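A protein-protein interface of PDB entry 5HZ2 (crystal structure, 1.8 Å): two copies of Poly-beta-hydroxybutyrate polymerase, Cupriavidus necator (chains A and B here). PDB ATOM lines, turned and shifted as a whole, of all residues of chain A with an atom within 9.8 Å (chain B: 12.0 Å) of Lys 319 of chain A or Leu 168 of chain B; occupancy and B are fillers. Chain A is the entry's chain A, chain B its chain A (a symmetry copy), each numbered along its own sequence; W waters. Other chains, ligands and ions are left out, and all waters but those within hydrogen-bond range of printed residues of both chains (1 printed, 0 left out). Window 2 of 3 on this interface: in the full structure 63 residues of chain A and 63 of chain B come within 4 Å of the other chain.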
ATOM      1  N   GLY A 303      -0.234 -11.745 -11.888  1.00  0.00           N
ATOM      2  CA  GLY A 303      -0.621 -12.383 -10.663  1.00  0.00           C
ATOM      3  C   GLY A 303       0.301 -13.543 -10.389  1.00  0.00           C
ATOM      4  O   GLY A 303       0.822 -14.138 -11.283  1.00  0.00           O
ATOM      5  N   ALA A 304       0.493 -13.851  -9.128  1.00  0.00           N
ATOM      6  CA  ALA A 304       1.320 -14.969  -8.759  1.00  0.00           C
ATOM      7  C   ALA A 304       0.574 -16.263  -9.024  1.00  0.00           C
ATOM      8  O   ALA A 304      -0.629 -16.277  -9.137  1.00  0.00           O
ATOM      9  CB  ALA A 304       1.701 -14.886  -7.294  1.00  0.00           C
ATOM     10  N   SER A 305       1.327 -17.344  -9.116  1.00  0.00           N
ATOM     11  CA  SER A 305       0.795 -18.683  -9.275  1.00  0.00           C
ATOM     12  C   SER A 305       0.335 -19.148 -10.665  1.00  0.00           C
ATOM     13  O   SER A 305       0.641 -18.538 -11.659  1.00  0.00           O
ATOM     14  CB  SER A 305      -0.258 -18.963  -8.191  1.00  0.00           C
ATOM     15  OG  SER A 305      -0.396 -20.333  -7.924  1.00  0.00           O
ATOM     16  N   ALA A 309      -5.261 -20.904 -10.313  1.00  0.00           N
ATOM     17  CA  ALA A 309      -4.959 -20.346  -8.981  1.00  0.00           C
ATOM     18  C   ALA A 309      -4.628 -18.885  -8.981  1.00  0.00           C
ATOM     19  O   ALA A 309      -5.021 -18.193  -8.068  1.00  0.00           O
ATOM     20  CB  ALA A 309      -3.893 -21.197  -8.248  1.00  0.00           C
ATOM     21  N   GLY A 310      -3.980 -18.382 -10.045  1.00  0.00           N
ATOM     22  CA  GLY A 310      -3.583 -17.000 -10.080  1.00  0.00           C
ATOM     23  C   GLY A 310      -4.720 -16.090 -10.432  1.00  0.00           C
ATOM     24  O   GLY A 310      -4.858 -14.978  -9.918  1.00  0.00           O
ATOM     25  N   VAL A 311      -5.547 -16.546 -11.366  1.00  0.00           N
ATOM     26  CA  VAL A 311      -6.699 -15.712 -11.797  1.00  0.00           C
ATOM     27  C   VAL A 311      -7.843 -15.773 -10.773  1.00  0.00           C
ATOM     28  O   VAL A 311      -8.458 -14.726 -10.443  1.00  0.00           O
ATOM     29  CB  VAL A 311      -7.021 -16.015 -13.310  1.00  0.00           C
ATOM     30  CG1 VAL A 311      -7.705 -17.302 -13.471  1.00  0.00           C
ATOM     31  CG2 VAL A 311      -7.849 -14.876 -13.953  1.00  0.00           C
ATOM     32  N   ILE A 312      -8.129 -16.971 -10.233  1.00  0.00           N
ATOM     33  CA  ILE A 312      -9.210 -17.126  -9.245  1.00  0.00           C
ATOM     34  C   ILE A 312      -8.667 -17.022  -7.853  1.00  0.00           C
ATOM     35  O   ILE A 312      -8.502 -18.035  -7.163  1.00  0.00           O
ATOM     36  CB  ILE A 312     -10.076 -18.438  -9.421  1.00  0.00           C
ATOM     37  CG1 ILE A 312     -10.519 -18.631 -10.889  1.00  0.00           C
ATOM     38  CG2 ILE A 312     -11.310 -18.371  -8.534  1.00  0.00           C
ATOM     39  CD1 ILE A 312     -11.227 -17.438 -11.492  1.00  0.00           C
ATOM     40  N   ASN A 313      -8.342 -15.798  -7.464  1.00  0.00           N
ATOM     41  CA  ASN A 313      -7.746 -15.487  -6.175  1.00  0.00           C
ATOM     42  C   ASN A 313      -8.534 -14.367  -5.478  1.00  0.00           C
ATOM     43  O   ASN A 313      -8.191 -13.202  -5.566  1.00  0.00           O
ATOM     44  CB  ASN A 313      -6.274 -15.114  -6.311  1.00  0.00           C
ATOM     45  CG  ASN A 313      -5.645 -14.812  -4.947  1.00  0.00           C
ATOM     46  OD1 ASN A 313      -6.142 -15.290  -3.952  1.00  0.00           O
ATOM     47  ND2 ASN A 313      -4.559 -14.010  -4.899  1.00  0.00           N
ATOM     48  N   PRO A 314      -9.642 -14.713  -4.785  1.00  0.00           N
ATOM     49  CA  PRO A 314     -10.482 -13.681  -4.213  1.00  0.00           C
ATOM     50  C   PRO A 314      -9.811 -12.952  -3.079  1.00  0.00           C
ATOM     51  O   PRO A 314      -9.115 -13.584  -2.277  1.00  0.00           O
ATOM     52  CB  PRO A 314     -11.721 -14.441  -3.675  1.00  0.00           C
ATOM     53  CG  PRO A 314     -11.506 -15.869  -4.003  1.00  0.00           C
ATOM     54  CD  PRO A 314     -10.056 -16.069  -4.390  1.00  0.00           C
ATOM     55  N   PRO A 315     -10.009 -11.649  -2.987  1.00  0.00           N
ATOM     56  CA  PRO A 315      -9.267 -10.869  -1.970  1.00  0.00           C
ATOM     57  C   PRO A 315      -9.514 -11.237  -0.514  1.00  0.00           C
ATOM     58  O   PRO A 315      -8.589 -11.089   0.306  1.00  0.00           O
ATOM     59  CB  PRO A 315      -9.642  -9.417  -2.244  1.00  0.00           C
ATOM     60  CG  PRO A 315     -10.711  -9.434  -3.237  1.00  0.00           C
ATOM     61  CD  PRO A 315     -10.813 -10.790  -3.868  1.00  0.00           C
ATOM     62  N   ALA A 316     -10.691 -11.787  -0.209  1.00  0.00           N
ATOM     63  CA  ALA A 316     -11.065 -12.097   1.199  1.00  0.00           C
ATOM     64  C   ALA A 316     -10.076 -13.065   1.837  1.00  0.00           C
ATOM     65  O   ALA A 316      -9.751 -12.915   2.989  1.00  0.00           O
ATOM     66  CB  ALA A 316     -12.485 -12.672   1.297  1.00  0.00           C
ATOM     67  N   LYS A 317      -9.520 -13.972   1.038  1.00  0.00           N
ATOM     68  CA  LYS A 317      -8.624 -15.000   1.526  1.00  0.00           C
ATOM     69  C   LYS A 317      -7.251 -14.415   1.826  1.00  0.00           C
ATOM     70  O   LYS A 317      -6.421 -15.049   2.464  1.00  0.00           O
ATOM     71  CB  LYS A 317      -8.550 -16.109   0.480  1.00  0.00           C
ATOM     72  CG  LYS A 317      -9.925 -16.693   0.212  1.00  0.00           C
ATOM     73  CD  LYS A 317      -9.868 -18.048  -0.466  1.00  0.00           C
ATOM     74  CE  LYS A 317     -11.250 -18.723  -0.417  1.00  0.00           C
ATOM     75  NZ  LYS A 317     -11.657 -19.305  -1.737  1.00  0.00           N
ATOM     76  N   ASN A 318      -6.981 -13.217   1.351  1.00  0.00           N
ATOM     77  CA  ASN A 318      -5.700 -12.616   1.650  1.00  0.00           C
ATOM     78  C   ASN A 318      -4.471 -13.468   1.299  1.00  0.00           C
ATOM     79  O   ASN A 318      -3.538 -13.568   2.079  1.00  0.00           O
ATOM     80  CB  ASN A 318      -5.673 -12.291   3.132  1.00  0.00           C
ATOM     81  CG  ASN A 318      -4.829 -11.104   3.433  1.00  0.00           C
ATOM     82  OD1 ASN A 318      -4.835 -10.137   2.694  1.00  0.00           O
ATOM     83  ND2 ASN A 318      -4.096 -11.167   4.518  1.00  0.00           N
ATOM     84  N   LYS A 319      -4.479 -14.076   0.127  1.00  0.00           N
ATOM     85  CA  LYS A 319      -3.394 -14.942  -0.283  1.00  0.00           C
ATOM     86  C   LYS A 319      -2.707 -14.452  -1.538  1.00  0.00           C
ATOM     87  O   LYS A 319      -3.253 -13.682  -2.287  1.00  0.00           O
ATOM     88  CB  LYS A 319      -3.917 -16.340  -0.553  1.00  0.00           C
ATOM     89  CG  LYS A 319      -4.630 -16.995   0.603  1.00  0.00           C
ATOM     90  CD  LYS A 319      -3.647 -17.593   1.575  1.00  0.00           C
ATOM     91  CE  LYS A 319      -4.358 -18.278   2.731  1.00  0.00           C
ATOM     92  NZ  LYS A 319      -5.406 -19.214   2.254  1.00  0.00           N
ATOM     93  N   ARG A 320      -1.484 -14.919  -1.717  1.00  0.00           N
ATOM     94  CA  ARG A 320      -0.657 -14.622  -2.867  1.00  0.00           C
ATOM     95  C   ARG A 320      -0.212 -13.169  -3.004  1.00  0.00           C
ATOM     96  O   ARG A 320      -0.137 -12.455  -2.041  1.00  0.00           O
ATOM     97  CB  ARG A 320      -1.282 -15.186  -4.149  1.00  0.00           C
ATOM     98  CG  ARG A 320      -1.844 -16.581  -3.974  1.00  0.00           C
ATOM     99  CD  ARG A 320      -2.043 -17.316  -5.277  1.00  0.00           C
ATOM    100  NE  ARG A 320      -2.563 -18.655  -5.086  1.00  0.00           N
ATOM    101  CZ  ARG A 320      -1.830 -19.725  -4.798  1.00  0.00           C
ATOM    102  NH1 ARG A 320      -0.525 -19.642  -4.647  1.00  0.00           N
ATOM    103  NH2 ARG A 320      -2.415 -20.884  -4.649  1.00  0.00           N
ATOM    104  N   SER A 321       0.084 -12.763  -4.225  1.00  0.00           N
ATOM    105  CA  SER A 321       0.590 -11.423  -4.519  1.00  0.00           C
ATOM    106  C   SER A 321       0.416 -11.190  -5.996  1.00  0.00           C
ATOM    107  O   SER A 321      -0.039 -12.080  -6.697  1.00  0.00           O
ATOM    108  CB  SER A 321       2.083 -11.349  -4.185  1.00  0.00           C
ATOM    109  OG  SER A 321       2.835 -12.304  -4.954  1.00  0.00           O
ATOM    110  N   HIS A 322       0.695  -9.962  -6.435  1.00  0.00           N
ATOM    111  CA  HIS A 322       0.670  -9.582  -7.845  1.00  0.00           C
ATOM    112  C   HIS A 322       1.700  -8.464  -8.050  1.00  0.00           C
ATOM    113  O   HIS A 322       2.137  -7.857  -7.091  1.00  0.00           O
ATOM    114  CB  HIS A 322      -0.745  -9.137  -8.269  1.00  0.00           C
ATOM    115  CG  HIS A 322      -1.278  -8.006  -7.438  1.00  0.00           C
ATOM    116  ND1 HIS A 322      -1.432  -6.725  -7.920  1.00  0.00           N
ATOM    117  CD2 HIS A 322      -1.696  -7.988  -6.165  1.00  0.00           C
ATOM    118  CE1 HIS A 322      -1.928  -5.958  -6.965  1.00  0.00           C
ATOM    119  NE2 HIS A 322      -2.097  -6.709  -5.885  1.00  0.00           N
ATOM    120  N   GLU A 341       6.042  -5.792  -6.381  1.00  0.00           N
ATOM    121  CA  GLU A 341       5.229  -6.835  -5.862  1.00  0.00           C
ATOM    122  C   GLU A 341       4.316  -6.283  -4.733  1.00  0.00           C
ATOM    123  O   GLU A 341       4.785  -5.582  -3.829  1.00  0.00           O
ATOM    124  CB  GLU A 341       6.074  -7.951  -5.252  1.00  0.00           C
ATOM    125  CG  GLU A 341       5.230  -9.193  -5.028  1.00  0.00           C
ATOM    126  CD  GLU A 341       6.007 -10.430  -4.633  1.00  0.00           C
ATOM    127  OE1 GLU A 341       7.253 -10.370  -4.479  1.00  0.00           O
ATOM    128  OE2 GLU A 341       5.348 -11.464  -4.491  1.00  0.00           O
ATOM    129  N   HIS A 342       3.033  -6.601  -4.828  1.00  0.00           N
ATOM    130  CA  HIS A 342       2.016  -6.170  -3.888  1.00  0.00           C
ATOM    131  C   HIS A 342       1.354  -7.369  -3.269  1.00  0.00           C
ATOM    132  O   HIS A 342       1.138  -8.364  -3.917  1.00  0.00           O
ATOM    133  CB  HIS A 342       0.933  -5.345  -4.573  1.00  0.00           C
ATOM    134  CG  HIS A 342       1.433  -4.078  -5.175  1.00  0.00           C
ATOM    135  ND1 HIS A 342       1.680  -3.942  -6.517  1.00  0.00           N
ATOM    136  CD2 HIS A 342       1.738  -2.890  -4.615  1.00  0.00           C
ATOM    137  CE1 HIS A 342       2.122  -2.727  -6.761  1.00  0.00           C
ATOM    138  NE2 HIS A 342       2.163  -2.066  -5.623  1.00  0.00           N
ATOM    139  N   HIS A 343       1.041  -7.268  -1.999  1.00  0.00           N
ATOM    140  CA  HIS A 343       0.410  -8.359  -1.319  1.00  0.00           C
ATOM    141  C   HIS A 343      -1.013  -8.639  -1.787  1.00  0.00           C
ATOM    142  O   HIS A 343      -1.756  -7.751  -2.118  1.00  0.00           O
ATOM    143  CB  HIS A 343       0.416  -8.129   0.185  1.00  0.00           C
ATOM    144  CG  HIS A 343      -0.162  -9.265   0.961  1.00  0.00           C
ATOM    145  ND1 HIS A 343       0.546 -10.410   1.237  1.00  0.00           N
ATOM    146  CD2 HIS A 343      -1.393  -9.447   1.485  1.00  0.00           C
ATOM    147  CE1 HIS A 343      -0.221 -11.246   1.909  1.00  0.00           C
ATOM    148  NE2 HIS A 343      -1.402 -10.685   2.070  1.00  0.00           N
ATOM    149  N   GLY A 344      -1.360  -9.904  -1.797  1.00  0.00           N
ATOM    150  CA  GLY A 344      -2.692 -10.330  -2.106  1.00  0.00           C
ATOM    151  C   GLY A 344      -3.185 -10.304  -3.516  1.00  0.00           C
ATOM    152  O   GLY A 344      -2.431 -10.195  -4.450  1.00  0.00           O
ATOM    153  N   SER A 345      -4.499 -10.406  -3.618  1.00  0.00           N
ATOM    154  CA  SER A 345      -5.180 -10.472  -4.895  1.00  0.00           C
ATOM    155  C   SER A 345      -4.975  -9.230  -5.755  1.00  0.00           C
ATOM    156  O   SER A 345      -4.985  -8.119  -5.265  1.00  0.00           O
ATOM    157  CB  SER A 345      -6.700 -10.605  -4.601  1.00  0.00           C
ATOM    158  OG  SER A 345      -7.449 -10.668  -5.797  1.00  0.00           O
ATOM    159  N   TRP A 346      -5.005  -9.463  -7.060  1.00  0.00           N
ATOM    160  CA  TRP A 346      -4.998  -8.417  -8.056  1.00  0.00           C
ATOM    161  C   TRP A 346      -6.438  -7.917  -8.326  1.00  0.00           C
ATOM    162  O   TRP A 346      -6.603  -6.922  -8.988  1.00  0.00           O
ATOM    163  CB  TRP A 346      -4.393  -8.897  -9.377  1.00  0.00           C
ATOM    164  CG  TRP A 346      -5.086 -10.076  -9.968  1.00  0.00           C
ATOM    165  CD1 TRP A 346      -4.802 -11.373  -9.745  1.00  0.00           C
ATOM    166  CD2 TRP A 346      -6.179 -10.059 -10.884  1.00  0.00           C
ATOM    167  NE1 TRP A 346      -5.640 -12.170 -10.452  1.00  0.00           N
ATOM    168  CE2 TRP A 346      -6.507 -11.386 -11.157  1.00  0.00           C
ATOM    169  CE3 TRP A 346      -6.924  -9.045 -11.484  1.00  0.00           C
ATOM    170  CZ2 TRP A 346      -7.551 -11.733 -12.011  1.00  0.00           C
ATOM    171  CZ3 TRP A 346      -7.938  -9.389 -12.331  1.00  0.00           C
ATOM    172  CH2 TRP A 346      -8.243 -10.719 -12.594  1.00  0.00           C
ATOM    173  N   TRP A 347      -7.468  -8.609  -7.827  1.00  0.00           N
ATOM    174  CA  TRP A 347      -8.846  -8.190  -8.085  1.00  0.00           C
ATOM    175  C   TRP A 347      -9.107  -6.745  -7.771  1.00  0.00           C
ATOM    176  O   TRP A 347      -9.700  -6.056  -8.618  1.00  0.00           O
ATOM    177  CB  TRP A 347      -9.890  -9.124  -7.461  1.00  0.00           C
ATOM    178  CG  TRP A 347      -9.951 -10.496  -8.010  1.00  0.00           C
ATOM    179  CD1 TRP A 347      -9.041 -11.121  -8.885  1.00  0.00           C
ATOM    180  CD2 TRP A 347     -10.937 -11.478  -7.719  1.00  0.00           C
ATOM    181  NE1 TRP A 347      -9.455 -12.366  -9.162  1.00  0.00           N
ATOM    182  CE2 TRP A 347     -10.610 -12.630  -8.457  1.00  0.00           C
ATOM    183  CE3 TRP A 347     -12.077 -11.490  -6.899  1.00  0.00           C
ATOM    184  CZ2 TRP A 347     -11.360 -13.789  -8.388  1.00  0.00           C
ATOM    185  CZ3 TRP A 347     -12.850 -12.594  -6.875  1.00  0.00           C
ATOM    186  CH2 TRP A 347     -12.486 -13.768  -7.593  1.00  0.00           C
ATOM    187  N   PRO A 348      -8.630  -6.230  -6.605  1.00  0.00           N
ATOM    188  CA  PRO A 348      -8.935  -4.805  -6.290  1.00  0.00           C
ATOM    189  C   PRO A 348      -8.320  -3.772  -7.210  1.00  0.00           C
ATOM    190  O   PRO A 348      -8.910  -2.731  -7.516  1.00  0.00           O
ATOM    191  CB  PRO A 348      -8.479  -4.631  -4.849  1.00  0.00           C
ATOM    192  CG  PRO A 348      -8.461  -6.013  -4.275  1.00  0.00           C
ATOM    193  CD  PRO A 348      -8.234  -6.991  -5.416  1.00  0.00           C
ATOM    194  N   ASP B 162       1.407 -25.641 -10.239  1.00  0.00           N
ATOM    195  CA  ASP B 162       1.077 -24.456  -9.470  1.00  0.00           C
ATOM    196  C   ASP B 162      -0.429 -24.226  -9.270  1.00  0.00           C
ATOM    197  O   ASP B 162      -0.885 -23.106  -9.312  1.00  0.00           O
ATOM    198  CB  ASP B 162       1.788 -23.217 -10.023  1.00  0.00           C
ATOM    199  CG  ASP B 162       3.251 -23.143  -9.610  1.00  0.00           C
ATOM    200  OD1 ASP B 162       3.527 -22.777  -8.463  1.00  0.00           O
ATOM    201  OD2 ASP B 162       4.117 -23.456 -10.415  1.00  0.00           O
ATOM    202  N   GLU B 163      -1.185 -25.306  -9.112  1.00  0.00           N
ATOM    203  CA  GLU B 163      -2.621 -25.206  -8.861  1.00  0.00           C
ATOM    204  C   GLU B 163      -3.038 -25.447  -7.378  1.00  0.00           C
ATOM    205  O   GLU B 163      -4.147 -25.142  -7.001  1.00  0.00           O
ATOM    206  CB  GLU B 163      -3.436 -26.028  -9.852  1.00  0.00           C
ATOM    207  CG  GLU B 163      -3.306 -25.563 -11.297  1.00  0.00           C
ATOM    208  CD  GLU B 163      -3.943 -24.205 -11.590  1.00  0.00           C
ATOM    209  OE1 GLU B 163      -4.587 -23.612 -10.721  1.00  0.00           O
ATOM    210  OE2 GLU B 163      -3.785 -23.733 -12.712  1.00  0.00           O
ATOM    211  N   GLY B 164      -2.146 -25.961  -6.540  1.00  0.00           N
ATOM    212  CA  GLY B 164      -2.493 -26.124  -5.088  1.00  0.00           C
ATOM    213  C   GLY B 164      -2.911 -24.828  -4.341  1.00  0.00           C
ATOM    214  O   GLY B 164      -2.342 -23.751  -4.565  1.00  0.00           O
ATOM    215  N   HIS B 165      -3.866 -24.954  -3.424  1.00  0.00           N
ATOM    216  CA  HIS B 165      -4.189 -23.891  -2.469  1.00  0.00           C
ATOM    217  C   HIS B 165      -3.098 -23.608  -1.494  1.00  0.00           C
ATOM    218  O   HIS B 165      -2.249 -24.473  -1.152  1.00  0.00           O
ATOM    219  CB  HIS B 165      -5.459 -24.229  -1.660  1.00  0.00           C
ATOM    220  CG  HIS B 165      -6.691 -24.220  -2.472  1.00  0.00           C
ATOM    221  ND1 HIS B 165      -7.896 -24.703  -2.009  1.00  0.00           N
ATOM    222  CD2 HIS B 165      -6.919 -23.792  -3.744  1.00  0.00           C
ATOM    223  CE1 HIS B 165      -8.815 -24.552  -2.948  1.00  0.00           C
ATOM    224  NE2 HIS B 165      -8.246 -24.004  -4.004  1.00  0.00           N
ATOM    225  N   VAL B 166      -3.120 -22.387  -0.996  1.00  0.00           N
ATOM    226  CA  VAL B 166      -2.159 -21.981   0.027  1.00  0.00           C
ATOM    227  C   VAL B 166      -2.808 -22.433   1.333  1.00  0.00           C
ATOM    228  O   VAL B 166      -3.921 -21.998   1.686  1.00  0.00           O
ATOM    229  CB  VAL B 166      -1.926 -20.469   0.070  1.00  0.00           C
ATOM    230  CG1 VAL B 166      -0.918 -20.117   1.187  1.00  0.00           C
ATOM    231  CG2 VAL B 166      -1.448 -19.945  -1.263  1.00  0.00           C
ATOM    232  N   GLN B 167      -2.100 -23.283   2.049  1.00  0.00           N
ATOM    233  CA  GLN B 167      -2.580 -23.807   3.307  1.00  0.00           C
ATOM    234  C   GLN B 167      -2.124 -23.030   4.531  1.00  0.00           C
ATOM    235  O   GLN B 167      -0.981 -22.659   4.657  1.00  0.00           O
ATOM    236  CB  GLN B 167      -2.117 -25.246   3.466  1.00  0.00           C
ATOM    237  CG  GLN B 167      -2.582 -26.182   2.358  1.00  0.00           C
ATOM    238  CD  GLN B 167      -4.080 -26.243   2.230  1.00  0.00           C
ATOM    239  OE1 GLN B 167      -4.800 -25.912   3.154  1.00  0.00           O
ATOM    240  NE2 GLN B 167      -4.553 -26.673   1.081  1.00  0.00           N
ATOM    241  N   LEU B 168      -3.060 -22.765   5.421  1.00  0.00           N
ATOM    242  CA  LEU B 168      -2.749 -22.122   6.690  1.00  0.00           C
ATOM    243  C   LEU B 168      -2.720 -23.200   7.775  1.00  0.00           C
ATOM    244  O   LEU B 168      -2.516 -22.908   8.929  1.00  0.00           O
ATOM    245  CB  LEU B 168      -3.804 -21.090   7.060  1.00  0.00           C
ATOM    246  CG  LEU B 168      -3.955 -19.865   6.178  1.00  0.00           C
ATOM    247  CD1 LEU B 168      -5.363 -19.327   6.325  1.00  0.00           C
ATOM    248  CD2 LEU B 168      -2.951 -18.804   6.576  1.00  0.00           C
ATOM    249  N   ARG B 169      -2.932 -24.444   7.371  1.00  0.00           N
ATOM    250  CA  ARG B 169      -3.030 -25.585   8.240  1.00  0.00           C
ATOM    251  C   ARG B 169      -2.223 -26.747   7.729  1.00  0.00           C
ATOM    252  O   ARG B 169      -1.784 -26.772   6.583  1.00  0.00           O
ATOM    253  CB  ARG B 169      -4.485 -26.041   8.255  1.00  0.00           C
ATOM    254  CG  ARG B 169      -5.007 -26.309   6.849  1.00  0.00           C
ATOM    255  CD  ARG B 169      -6.131 -25.357   6.472  1.00  0.00           C
ATOM    256  NE  ARG B 169      -5.705 -24.285   5.581  1.00  0.00           N
ATOM    257  CZ  ARG B 169      -6.490 -23.281   5.209  1.00  0.00           C
ATOM    258  NH1 ARG B 169      -7.733 -23.219   5.648  1.00  0.00           N
ATOM    259  NH2 ARG B 169      -6.040 -22.342   4.401  1.00  0.00           N
ATOM    260  N   GLU B 170      -2.019 -27.727   8.597  1.00  0.00           N
ATOM    261  CA  GLU B 170      -1.314 -28.925   8.208  1.00  0.00           C
ATOM    262  C   GLU B 170      -2.212 -29.526   7.137  1.00  0.00           C
ATOM    263  O   GLU B 170      -3.432 -29.547   7.290  1.00  0.00           O
ATOM    264  CB  GLU B 170      -1.216 -29.876   9.399  1.00  0.00           C
ATOM    265  CG  GLU B 170      -0.576 -31.218   9.095  1.00  0.00           C
ATOM    266  CD  GLU B 170      -1.558 -32.366   9.198  1.00  0.00           C
ATOM    267  OE1 GLU B 170      -2.518 -32.259   9.988  1.00  0.00           O
ATOM    268  OE2 GLU B 170      -1.374 -33.370   8.485  1.00  0.00           O
ATOM    269  N   ALA B 171      -1.624 -29.987   6.049  1.00  0.00           N
ATOM    270  CA  ALA B 171      -2.410 -30.571   4.990  1.00  0.00           C
ATOM    271  C   ALA B 171      -1.673 -31.774   4.469  1.00  0.00           C
ATOM    272  O   ALA B 171      -0.462 -31.882   4.614  1.00  0.00           O
ATOM    273  CB  ALA B 171      -2.672 -29.564   3.887  1.00  0.00           C
ATOM    274  N   THR B 172      -2.408 -32.695   3.876  1.00  0.00           N
ATOM    275  CA  THR B 172      -1.795 -33.897   3.360  1.00  0.00           C
ATOM    276  C   THR B 172      -2.362 -34.195   2.000  1.00  0.00           C
ATOM    277  O   THR B 172      -3.450 -33.766   1.665  1.00  0.00           O
ATOM    278  CB  THR B 172      -2.057 -35.110   4.276  1.00  0.00           C
ATOM    279  OG1 THR B 172      -1.430 -36.272   3.727  1.00  0.00           O
ATOM    280  CG2 THR B 172      -3.531 -35.375   4.385  1.00  0.00           C
HETATM  281  O   HOH W   1       1.761 -21.308  -6.818  1.00  0.00           O
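The backbone carbonyl oxygen (O) of Asp 162 of chain B lies within hydrogen-bond range of the side-chain hydroxyl (OG) of Ser 305 of chain A. The backbone NH of Ala 309 of chain A sits at hydrogen-bond distance from the side-chain carboxylate of Glu 163 of chain B (2.8 Å). The backbone carbonyl oxygen of Val 166 of chain B lies within hydrogen-bond range of the side-chain amino group of Lys 319 of chain A. The backbone carbonyl oxygen of Gly 164 of chain B is in hydrogen-bond range of the guanidinium group of Arg 320 of chain A (2.9 Å).
The side-chain hydroxyl (OG) of Ser 305 of chain A sits at hydrogen-bond distance from the guanidinium group (NH1) of Arg 320 of chain A. O of Lys 319 of chain A lies within hydrogen-bond range of ND2 of Asn 313 of chain A. The backbone NH of Gly 344 of chain A is in hydrogen-bond range of the backbone carbonyl oxygen of Arg 320 of chain A (2.8 Å). The guanidinium group (NH2) of Arg 169 of chain B is in hydrogen-bond range of the backbone carbonyl oxygen (O) of Val 166 of chain B (3.5 Å). The guanidinium group of Arg 169 of chain B is in hydrogen-bond range of the side-chain amide oxygen of Gln 167 of chain B, 3.1 Å away.
Among the printed residues, pairs that only touch across the chains: Arg 320 of chain A with Val 166 of chain B (3.5 Å), Ala 309 of chain A with Asp 162 of chain B (3.7 Å), Lys 319 of chain A with Leu 168 of chain B (3.8 Å) and Lys 319 of chain A with Arg 169 of chain B (3.8 Å).
Lys 319 of chain A touches just these residues of chain B: Val 166, Leu 168 and Arg 169. Leu 168 of chain B touches just one residue of chain A: Lys 319 (3.8 Å). No residue of chain B comes within 4 Å of Asn 313 of chain A. No residue of chain B comes within 4 Å of Lys 317 of chain A. No residue of chain B comes within 4 Å of Asn 318 of chain A. No residue of chain B comes within 4 Å of Ser 321 of chain A. No residue of chain B comes within 4 Å of His 343 of chain A. No residue of chain B comes within 4 Å of Gly 344 of chain A. No residue of chain B comes within 4 Å of Ser 345 of chain A. Val 166 of chain B touches just these residues of chain A: Lys 319 and Arg 320. Arg 169 of chain B touches just one residue of chain A: Lys 319 (3.8 Å). Of the printed residues of chain A, Asp 162 of chain B touches Ser 305 (3.1 Å) and Ala 309 (3.7 Å). Of the printed residues of chain A, Gly 164 of chain B touches Arg 320 (2.9 Å). Of the printed residues of chain A, Glu 163 of chain B touches Ala 309 (2.8 Å). Ala 304 of chain A touches none of the printed residues of chain B. Thr 172 of chain B touches none of the printed residues of chain A. The nearest residue of chain B that does not touch Lys 319 of chain A is Gln 167 of chain B (5.2 Å). The nearest residue of chain A that does not touch Leu 168 of chain B is Lys 317 of chain A (5.9 Å). The nearest printed residue of chain A that does not touch Asp 162 of chain B is Arg 320 of chain A (5.4 Å).
Of the 11 printed residues of chain B, 6 touch a printed residue of chain A. Printed residues of chain B that touch a printed residue of chain A: Asp 162, Glu 163, Gly 164, Val 166, Leu 168 and Arg 169. Of the 25 printed residues of chain A, 4 touch a printed residue of chain B. Printed residues of chain A that touch a printed residue of chain B: Ser 305, Ala 309, Lys 319 and Arg 320. Among the printed residues, no Asp or Glu carboxylate lies within 4 Å of a Lys or Arg side-chain nitrogen of the other chain.
No position is printed for both chains. Of the 8 pairs that touch across the chains among the printed residues, none has its exchanged pair printed and touching as well.
Water W1 bridges OG of Ser 305 of chain A (2.6 Å) and OD1 of Asp 162 of chain B (2.8 Å).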
